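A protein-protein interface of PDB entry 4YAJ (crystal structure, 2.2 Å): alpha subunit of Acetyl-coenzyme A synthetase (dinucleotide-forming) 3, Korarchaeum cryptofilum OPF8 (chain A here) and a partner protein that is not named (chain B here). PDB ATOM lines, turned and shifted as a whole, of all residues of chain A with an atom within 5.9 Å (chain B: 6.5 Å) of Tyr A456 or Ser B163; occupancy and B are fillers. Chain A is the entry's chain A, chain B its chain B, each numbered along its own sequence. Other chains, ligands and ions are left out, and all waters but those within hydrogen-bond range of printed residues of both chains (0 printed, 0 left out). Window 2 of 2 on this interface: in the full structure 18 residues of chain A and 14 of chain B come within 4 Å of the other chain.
The side-chain hydroxyl (OG) of Ser B163 sits at hydrogen-bond distance from the guanidinium group (NH2) of Arg B152 (2.8 Å). OE1 of Glu B167 is in salt-bridge range of NH1 of Arg B152. The side-chain hydroxyl of Ser B157 sits close to the backbone NH of Gln B159 (3.3 Å). N of Asp B160 is in hydrogen-bond range of OG of Ser B157 (2.9 Å). O of Gln B159 sits at hydrogen-bond distance from OG of Ser B163 (2.9 Å). The backbone carbonyl oxygen of Asp B160 lies within hydrogen-bond range of the side-chain hydroxyl of Ser B163 (3.1 Å).
Printed residues of chain A that touch a printed residue of chain B: Lys A270, Gln A271, Tyr A456, Lys A459 and Ser A460. Hydrophobic or aromatic side chains of chain A within 4 Å of the printed part of chain B: Tyr A456. Among the printed residues, 12 pairs touch across the chains.
Printed residues of chain B within 4 Å of Tyr A456: Arg B152 (3.2 Å), Gln B159 (3.4 Å), Asp B160 (2.9 Å) and Ser B163 (3.0 Å). Ser B163 touches just one residue of chain A: Tyr A456. Printed residues of chain B within 4 Å of Lys A270: Arg B152 (3.4 Å) and Glu B167 (2.7 Å). Printed residues of chain A within 4 Å of Ser B157: Ser A460. Of the printed residues of chain A, Arg B152 touches Lys A270 (3.4 Å), Gln A271 (3.6 Å) and Tyr A456 (3.2 Å). Ser A455 touches none of the printed residues of chain B. The nearest residue of chain A that does not touch Ser B163 is Lys A270 (5.1 Å).
The side-chain amino group (NZ) of Lys A270 is in salt-bridge range of the side-chain carboxylate (OE1) of Glu B167 (2.7 Å). The guanidinium group (NE) of Arg B152 is in hydrogen-bond range of the side-chain hydroxyl (OH) of Tyr A456, 3.2 Å away. OH of Tyr A456 sits at hydrogen-bond distance from OD1 of Asp B160, at 2.9 Å. The side-chain hydroxyl (OG) of Ser B163 sits at hydrogen-bond distance from the side-chain hydroxyl (OH) of Tyr A456, at 3.0 Å. The side-chain hydroxyl (OG) of Ser A460 sits at hydrogen-bond distance from the side-chain hydroxyl (OG) of Ser B157, at 2.9 Å. The side-chain hydroxyl (OG) of Ser A460 is in hydrogen-bond range of the side-chain carboxylate (OD2) of Asp B160, at 3.5 Å. NH2 of Arg B152 lies close to NZ of Lys A270 (3.4 Å).
Among the printed residues, pairs that only touch across the chains: Gln A271 with Arg B152 (3.6 Å), Gln A271 with Asp B160 (3.5 Å), Tyr A456 with Gln B159 (3.4 Å), Lys A459 with Gln B159 (3.9 Å) and Ser A460 with Gln B159 (3.97 Å).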
ATOM      1  N   LYS A 270     -13.730 -35.062  25.168  1.00  0.00           N
ATOM      2  CA  LYS A 270     -13.793 -33.680  24.709  1.00  0.00           C
ATOM      3  C   LYS A 270     -12.390 -33.101  24.523  1.00  0.00           C
ATOM      4  O   LYS A 270     -12.101 -32.431  23.533  1.00  0.00           O
ATOM      5  CB  LYS A 270     -14.568 -32.818  25.706  1.00  0.00           C
ATOM      6  CG  LYS A 270     -14.835 -31.396  25.218  1.00  0.00           C
ATOM      7  CD  LYS A 270     -15.586 -30.544  26.243  1.00  0.00           C
ATOM      8  CE  LYS A 270     -16.833 -31.217  26.792  1.00  0.00           C
ATOM      9  NZ  LYS A 270     -17.537 -30.339  27.766  1.00  0.00           N
ATOM     10  N   GLN A 271     -11.512 -33.372  25.482  1.00  0.00           N
ATOM     11  CA  GLN A 271     -10.148 -32.859  25.423  1.00  0.00           C
ATOM     12  C   GLN A 271      -9.348 -33.536  24.318  1.00  0.00           C
ATOM     13  O   GLN A 271      -8.316 -33.027  23.892  1.00  0.00           O
ATOM     14  CB  GLN A 271      -9.453 -33.045  26.772  1.00  0.00           C
ATOM     15  CG  GLN A 271     -10.081 -32.237  27.891  1.00  0.00           C
ATOM     16  CD  GLN A 271      -9.519 -32.587  29.255  1.00  0.00           C
ATOM     17  OE1 GLN A 271     -10.184 -33.231  30.062  1.00  0.00           O
ATOM     18  NE2 GLN A 271      -8.295 -32.150  29.521  1.00  0.00           N
ATOM     19  N   GLY A 273     -10.828 -34.261  21.396  1.00  0.00           N
ATOM     20  CA  GLY A 273     -11.488 -33.879  20.162  1.00  0.00           C
ATOM     21  C   GLY A 273     -12.319 -35.004  19.572  1.00  0.00           C
ATOM     22  O   GLY A 273     -12.685 -34.961  18.399  1.00  0.00           O
ATOM     23  N   ALA A 451     -15.330 -30.384  13.191  1.00  0.00           N
ATOM     24  CA  ALA A 451     -14.664 -29.107  12.968  1.00  0.00           C
ATOM     25  C   ALA A 451     -14.491 -28.355  14.286  1.00  0.00           C
ATOM     26  O   ALA A 451     -13.435 -27.792  14.559  1.00  0.00           O
ATOM     27  CB  ALA A 451     -15.445 -28.266  11.974  1.00  0.00           C
ATOM     28  N   ARG A 452     -15.532 -28.362  15.110  1.00  0.00           N
ATOM     29  CA  ARG A 452     -15.484 -27.674  16.394  1.00  0.00           C
ATOM     30  C   ARG A 452     -14.583 -28.393  17.398  1.00  0.00           C
ATOM     31  O   ARG A 452     -13.851 -27.752  18.145  1.00  0.00           O
ATOM     32  CB  ARG A 452     -16.894 -27.524  16.960  1.00  0.00           C
ATOM     33  CG  ARG A 452     -17.759 -26.565  16.161  1.00  0.00           C
ATOM     34  CD  ARG A 452     -19.210 -26.593  16.610  1.00  0.00           C
ATOM     35  NE  ARG A 452     -20.032 -25.663  15.841  1.00  0.00           N
ATOM     36  CZ  ARG A 452     -21.356 -25.578  15.929  1.00  0.00           C
ATOM     37  NH1 ARG A 452     -22.027 -26.370  16.755  1.00  0.00           N
ATOM     38  NH2 ARG A 452     -22.015 -24.695  15.191  1.00  0.00           N
ATOM     39  N   ALA A 453     -14.624 -29.720  17.400  1.00  0.00           N
ATOM     40  CA  ALA A 453     -13.772 -30.506  18.287  1.00  0.00           C
ATOM     41  C   ALA A 453     -12.304 -30.270  17.960  1.00  0.00           C
ATOM     42  O   ALA A 453     -11.464 -30.112  18.842  1.00  0.00           O
ATOM     43  CB  ALA A 453     -14.105 -31.981  18.168  1.00  0.00           C
ATOM     44  N   ARG A 454     -12.009 -30.251  16.670  1.00  0.00           N
ATOM     45  CA  ARG A 454     -10.660 -30.024  16.185  1.00  0.00           C
ATOM     46  C   ARG A 454     -10.185 -28.625  16.569  1.00  0.00           C
ATOM     47  O   ARG A 454      -9.033 -28.436  16.960  1.00  0.00           O
ATOM     48  CB  ARG A 454     -10.622 -30.278  14.680  1.00  0.00           C
ATOM     49  CG  ARG A 454      -9.268 -30.141  14.028  1.00  0.00           C
ATOM     50  CD  ARG A 454      -9.257 -30.923  12.722  1.00  0.00           C
ATOM     51  NE  ARG A 454      -9.216 -30.132  11.500  1.00  0.00           N
ATOM     52  CZ  ARG A 454      -9.006 -30.665  10.301  1.00  0.00           C
ATOM     53  NH1 ARG A 454      -8.806 -31.974  10.183  1.00  0.00           N
ATOM     54  NH2 ARG A 454      -8.985 -29.898   9.219  1.00  0.00           N
ATOM     55  N   SER A 455     -11.081 -27.649  16.466  1.00  0.00           N
ATOM     56  CA  SER A 455     -10.773 -26.286  16.878  1.00  0.00           C
ATOM     57  C   SER A 455     -10.488 -26.232  18.379  1.00  0.00           C
ATOM     58  O   SER A 455      -9.609 -25.495  18.825  1.00  0.00           O
ATOM     59  CB  SER A 455     -11.923 -25.344  16.524  1.00  0.00           C
ATOM     60  OG  SER A 455     -11.771 -24.094  17.170  1.00  0.00           O
ATOM     61  N   TYR A 456     -11.246 -27.009  19.151  1.00  0.00           N
ATOM     62  CA  TYR A 456     -11.045 -27.104  20.594  1.00  0.00           C
ATOM     63  C   TYR A 456      -9.624 -27.560  20.900  1.00  0.00           C
ATOM     64  O   TYR A 456      -8.937 -26.963  21.728  1.00  0.00           O
ATOM     65  CB  TYR A 456     -12.054 -28.071  21.224  1.00  0.00           C
ATOM     66  CG  TYR A 456     -12.005 -28.134  22.737  1.00  0.00           C
ATOM     67  CD1 TYR A 456     -11.005 -28.841  23.393  1.00  0.00           C
ATOM     68  CD2 TYR A 456     -12.966 -27.497  23.507  1.00  0.00           C
ATOM     69  CE1 TYR A 456     -10.959 -28.901  24.771  1.00  0.00           C
ATOM     70  CE2 TYR A 456     -12.929 -27.552  24.885  1.00  0.00           C
ATOM     71  CZ  TYR A 456     -11.925 -28.255  25.512  1.00  0.00           C
ATOM     72  OH  TYR A 456     -11.897 -28.304  26.886  1.00  0.00           O
ATOM     73  N   VAL A 457      -9.192 -28.625  20.233  1.00  0.00           N
ATOM     74  CA  VAL A 457      -7.862 -29.175  20.464  1.00  0.00           C
ATOM     75  C   VAL A 457      -6.791 -28.161  20.069  1.00  0.00           C
ATOM     76  O   VAL A 457      -5.811 -27.981  20.792  1.00  0.00           O
ATOM     77  CB  VAL A 457      -7.654 -30.493  19.684  1.00  0.00           C
ATOM     78  CG1 VAL A 457      -6.211 -30.972  19.784  1.00  0.00           C
ATOM     79  CG2 VAL A 457      -8.593 -31.566  20.202  1.00  0.00           C
ATOM     80  N   MET A 458      -6.984 -27.494  18.934  1.00  0.00           N
ATOM     81  CA  MET A 458      -6.034 -26.487  18.471  1.00  0.00           C
ATOM     82  C   MET A 458      -5.850 -25.373  19.499  1.00  0.00           C
ATOM     83  O   MET A 458      -4.724 -25.022  19.856  1.00  0.00           O
ATOM     84  CB  MET A 458      -6.492 -25.890  17.139  1.00  0.00           C
ATOM     85  CG  MET A 458      -6.181 -26.752  15.924  1.00  0.00           C
ATOM     86  SD  MET A 458      -4.413 -26.963  15.621  1.00  0.00           S
ATOM     87  CE  MET A 458      -3.882 -25.269  15.369  1.00  0.00           C
ATOM     88  N   LYS A 459      -6.961 -24.829  19.983  1.00  0.00           N
ATOM     89  CA  LYS A 459      -6.904 -23.770  20.980  1.00  0.00           C
ATOM     90  C   LYS A 459      -6.236 -24.286  22.247  1.00  0.00           C
ATOM     91  O   LYS A 459      -5.424 -23.594  22.855  1.00  0.00           O
ATOM     92  CB  LYS A 459      -8.304 -23.237  21.287  1.00  0.00           C
ATOM     93  CG  LYS A 459      -8.930 -22.481  20.127  1.00  0.00           C
ATOM     94  CD  LYS A 459     -10.339 -22.013  20.444  1.00  0.00           C
ATOM     95  CE  LYS A 459     -10.951 -21.276  19.264  1.00  0.00           C
ATOM     96  NZ  LYS A 459     -12.294 -20.721  19.579  1.00  0.00           N
ATOM     97  N   SER A 460      -6.543 -25.528  22.604  1.00  0.00           N
ATOM     98  CA  SER A 460      -5.993 -26.137  23.805  1.00  0.00           C
ATOM     99  C   SER A 460      -4.478 -26.296  23.697  1.00  0.00           C
ATOM    100  O   SER A 460      -3.775 -26.287  24.705  1.00  0.00           O
ATOM    101  CB  SER A 460      -6.646 -27.499  24.051  1.00  0.00           C
ATOM    102  OG  SER A 460      -6.356 -27.969  25.353  1.00  0.00           O
ATOM    103  N   LEU A 461      -3.985 -26.428  22.469  1.00  0.00           N
ATOM    104  CA  LEU A 461      -2.557 -26.592  22.213  1.00  0.00           C
ATOM    105  C   LEU A 461      -1.855 -25.272  21.897  1.00  0.00           C
ATOM    106  O   LEU A 461      -0.665 -25.265  21.592  1.00  0.00           O
ATOM    107  CB  LEU A 461      -2.332 -27.575  21.061  1.00  0.00           C
ATOM    108  CG  LEU A 461      -2.741 -29.030  21.300  1.00  0.00           C
ATOM    109  CD1 LEU A 461      -2.511 -29.848  20.043  1.00  0.00           C
ATOM    110  CD2 LEU A 461      -1.985 -29.635  22.476  1.00  0.00           C
ATOM    111  N   SER B 150     -18.201 -29.824  36.760  1.00  0.00           N
ATOM    112  CA  SER B 150     -17.504 -30.141  35.518  1.00  0.00           C
ATOM    113  C   SER B 150     -16.106 -30.666  35.824  1.00  0.00           C
ATOM    114  O   SER B 150     -15.531 -30.344  36.860  1.00  0.00           O
ATOM    115  CB  SER B 150     -17.423 -28.910  34.613  1.00  0.00           C
ATOM    116  OG  SER B 150     -16.667 -27.877  35.219  1.00  0.00           O
ATOM    117  N   ARG B 152     -12.060 -31.629  34.156  1.00  0.00           N
ATOM    118  CA  ARG B 152     -11.040 -31.579  33.115  1.00  0.00           C
ATOM    119  C   ARG B 152      -9.770 -32.276  33.596  1.00  0.00           C
ATOM    120  O   ARG B 152      -9.308 -32.040  34.711  1.00  0.00           O
ATOM    121  CB  ARG B 152     -10.727 -30.134  32.719  1.00  0.00           C
ATOM    122  CG  ARG B 152     -11.828 -29.423  31.945  1.00  0.00           C
ATOM    123  CD  ARG B 152     -12.025 -30.024  30.560  1.00  0.00           C
ATOM    124  NE  ARG B 152     -12.937 -29.228  29.744  1.00  0.00           N
ATOM    125  CZ  ARG B 152     -14.262 -29.255  29.849  1.00  0.00           C
ATOM    126  NH1 ARG B 152     -14.851 -30.044  30.739  1.00  0.00           N
ATOM    127  NH2 ARG B 152     -15.003 -28.488  29.062  1.00  0.00           N
ATOM    128  N   SER B 157      -5.403 -26.385  29.926  1.00  0.00           N
ATOM    129  CA  SER B 157      -5.154 -25.248  29.053  1.00  0.00           C
ATOM    130  C   SER B 157      -6.134 -24.135  29.407  1.00  0.00           C
ATOM    131  O   SER B 157      -7.074 -24.347  30.174  1.00  0.00           O
ATOM    132  CB  SER B 157      -5.318 -25.639  27.588  1.00  0.00           C
ATOM    133  OG  SER B 157      -6.685 -25.877  27.321  1.00  0.00           O
ATOM    134  N   GLU B 158      -5.920 -22.954  28.839  1.00  0.00           N
ATOM    135  CA  GLU B 158      -6.862 -21.858  29.005  1.00  0.00           C
ATOM    136  C   GLU B 158      -8.219 -22.259  28.434  1.00  0.00           C
ATOM    137  O   GLU B 158      -9.265 -21.930  28.994  1.00  0.00           O
ATOM    138  CB  GLU B 158      -6.342 -20.593  28.320  1.00  0.00           C
ATOM    139  CG  GLU B 158      -7.284 -19.402  28.402  1.00  0.00           C
ATOM    140  CD  GLU B 158      -6.680 -18.137  27.822  1.00  0.00           C
ATOM    141  OE1 GLU B 158      -5.439 -18.064  27.703  1.00  0.00           O
ATOM    142  OE2 GLU B 158      -7.449 -17.211  27.488  1.00  0.00           O
ATOM    143  N   GLN B 159      -8.188 -22.987  27.322  1.00  0.00           N
ATOM    144  CA  GLN B 159      -9.402 -23.469  26.673  1.00  0.00           C
ATOM    145  C   GLN B 159     -10.135 -24.487  27.546  1.00  0.00           C
ATOM    146  O   GLN B 159     -11.362 -24.532  27.571  1.00  0.00           O
ATOM    147  CB  GLN B 159      -9.062 -24.085  25.313  1.00  0.00           C
ATOM    148  CG  GLN B 159     -10.242 -24.714  24.586  1.00  0.00           C
ATOM    149  CD  GLN B 159     -11.298 -23.699  24.191  1.00  0.00           C
ATOM    150  OE1 GLN B 159     -11.054 -22.493  24.200  1.00  0.00           O
ATOM    151  NE2 GLN B 159     -12.486 -24.185  23.860  1.00  0.00           N
ATOM    152  N   ASP B 160      -9.383 -25.323  28.254  1.00  0.00           N
ATOM    153  CA  ASP B 160      -9.986 -26.285  29.169  1.00  0.00           C
ATOM    154  C   ASP B 160     -10.703 -25.568  30.308  1.00  0.00           C
ATOM    155  O   ASP B 160     -11.850 -25.883  30.630  1.00  0.00           O
ATOM    156  CB  ASP B 160      -8.927 -27.235  29.734  1.00  0.00           C
ATOM    157  CG  ASP B 160      -8.446 -28.250  28.714  1.00  0.00           C
ATOM    158  OD1 ASP B 160      -9.282 -28.792  27.966  1.00  0.00           O
ATOM    159  OD2 ASP B 160      -7.224 -28.498  28.656  1.00  0.00           O
ATOM    160  N   ALA B 161     -10.025 -24.592  30.903  1.00  0.00           N
ATOM    161  CA  ALA B 161     -10.572 -23.871  32.047  1.00  0.00           C
ATOM    162  C   ALA B 161     -11.821 -23.084  31.667  1.00  0.00           C
ATOM    163  O   ALA B 161     -12.839 -23.146  32.355  1.00  0.00           O
ATOM    164  CB  ALA B 161      -9.525 -22.942  32.631  1.00  0.00           C
ATOM    165  N   GLU B 162     -11.749 -22.350  30.563  1.00  0.00           N
ATOM    166  CA  GLU B 162     -12.869 -21.523  30.138  1.00  0.00           C
ATOM    167  C   GLU B 162     -14.101 -22.376  29.847  1.00  0.00           C
ATOM    168  O   GLU B 162     -15.195 -22.082  30.329  1.00  0.00           O
ATOM    169  CB  GLU B 162     -12.491 -20.700  28.907  1.00  0.00           C
ATOM    170  CG  GLU B 162     -13.553 -19.692  28.491  1.00  0.00           C
ATOM    171  CD  GLU B 162     -13.045 -18.686  27.475  1.00  0.00           C
ATOM    172  OE1 GLU B 162     -11.987 -18.069  27.719  1.00  0.00           O
ATOM    173  OE2 GLU B 162     -13.706 -18.513  26.430  1.00  0.00           O
ATOM    174  N   SER B 163     -13.916 -23.438  29.069  1.00  0.00           N
ATOM    175  CA  SER B 163     -15.032 -24.279  28.654  1.00  0.00           C
ATOM    176  C   SER B 163     -15.658 -25.023  29.832  1.00  0.00           C
ATOM    177  O   SER B 163     -16.874 -25.207  29.873  1.00  0.00           O
ATOM    178  CB  SER B 163     -14.584 -25.276  27.585  1.00  0.00           C
ATOM    179  OG  SER B 163     -13.670 -26.221  28.107  1.00  0.00           O
ATOM    180  N   MET B 164     -14.844 -25.448  30.795  1.00  0.00           N
ATOM    181  CA  MET B 164     -15.385 -26.190  31.929  1.00  0.00           C
ATOM    182  C   MET B 164     -16.161 -25.253  32.852  1.00  0.00           C
ATOM    183  O   MET B 164     -17.101 -25.678  33.519  1.00  0.00           O
ATOM    184  CB  MET B 164     -14.278 -26.918  32.703  1.00  0.00           C
ATOM    185  CG  MET B 164     -13.507 -26.067  33.701  1.00  0.00           C
ATOM    186  SD  MET B 164     -12.161 -26.967  34.491  1.00  0.00           S
ATOM    187  CE  MET B 164     -13.062 -28.232  35.381  1.00  0.00           C
ATOM    188  N   ILE B 165     -15.781 -23.979  32.882  1.00  0.00           N
ATOM    189  CA  ILE B 165     -16.544 -22.994  33.640  1.00  0.00           C
ATOM    190  C   ILE B 165     -17.905 -22.764  32.990  1.00  0.00           C
ATOM    191  O   ILE B 165     -18.934 -22.834  33.656  1.00  0.00           O
ATOM    192  CB  ILE B 165     -15.791 -21.651  33.758  1.00  0.00           C
ATOM    193  CG1 ILE B 165     -14.581 -21.806  34.680  1.00  0.00           C
ATOM    194  CG2 ILE B 165     -16.713 -20.553  34.299  1.00  0.00           C
ATOM    195  CD1 ILE B 165     -13.661 -20.605  34.705  1.00  0.00           C
ATOM    196  N   LYS B 166     -17.910 -22.489  31.691  1.00  0.00           N
ATOM    197  CA  LYS B 166     -19.155 -22.209  30.981  1.00  0.00           C
ATOM    198  C   LYS B 166     -20.068 -23.432  30.902  1.00  0.00           C
ATOM    199  O   LYS B 166     -21.252 -23.308  30.599  1.00  0.00           O
ATOM    200  CB  LYS B 166     -18.860 -21.676  29.579  1.00  0.00           C
ATOM    201  CG  LYS B 166     -17.983 -20.438  29.590  1.00  0.00           C
ATOM    202  CD  LYS B 166     -17.898 -19.776  28.229  1.00  0.00           C
ATOM    203  CE  LYS B 166     -17.133 -18.464  28.317  1.00  0.00           C
ATOM    204  NZ  LYS B 166     -17.071 -17.751  27.013  1.00  0.00           N
ATOM    205  N   GLU B 167     -19.514 -24.606  31.181  1.00  0.00           N
ATOM    206  CA  GLU B 167     -20.228 -25.860  30.979  1.00  0.00           C
ATOM    207  C   GLU B 167     -21.283 -26.127  32.057  1.00  0.00           C
ATOM    208  O   GLU B 167     -22.316 -26.731  31.772  1.00  0.00           O
ATOM    209  CB  GLU B 167     -19.226 -27.018  30.929  1.00  0.00           C
ATOM    210  CG  GLU B 167     -19.847 -28.404  30.874  1.00  0.00           C
ATOM    211  CD  GLU B 167     -18.807 -29.506  30.833  1.00  0.00           C
ATOM    212  OE1 GLU B 167     -17.745 -29.302  30.208  1.00  0.00           O
ATOM    213  OE2 GLU B 167     -19.048 -30.575  31.430  1.00  0.00           O
ATOM    214  N   VAL B 168     -21.035 -25.682  33.284  1.00  0.00           N
ATOM    215  CA  VAL B 168     -21.929 -26.004  34.397  1.00  0.00           C
ATOM    216  C   VAL B 168     -23.265 -25.268  34.291  1.00  0.00           C
ATOM    217  O   VAL B 168     -23.340 -24.153  33.775  1.00  0.00           O
ATOM    218  CB  VAL B 168     -21.277 -25.686  35.762  1.00  0.00           C
ATOM    219  CG1 VAL B 168     -19.992 -26.480  35.925  1.00  0.00           C
ATOM    220  CG2 VAL B 168     -21.007 -24.201  35.910  1.00  0.00           C
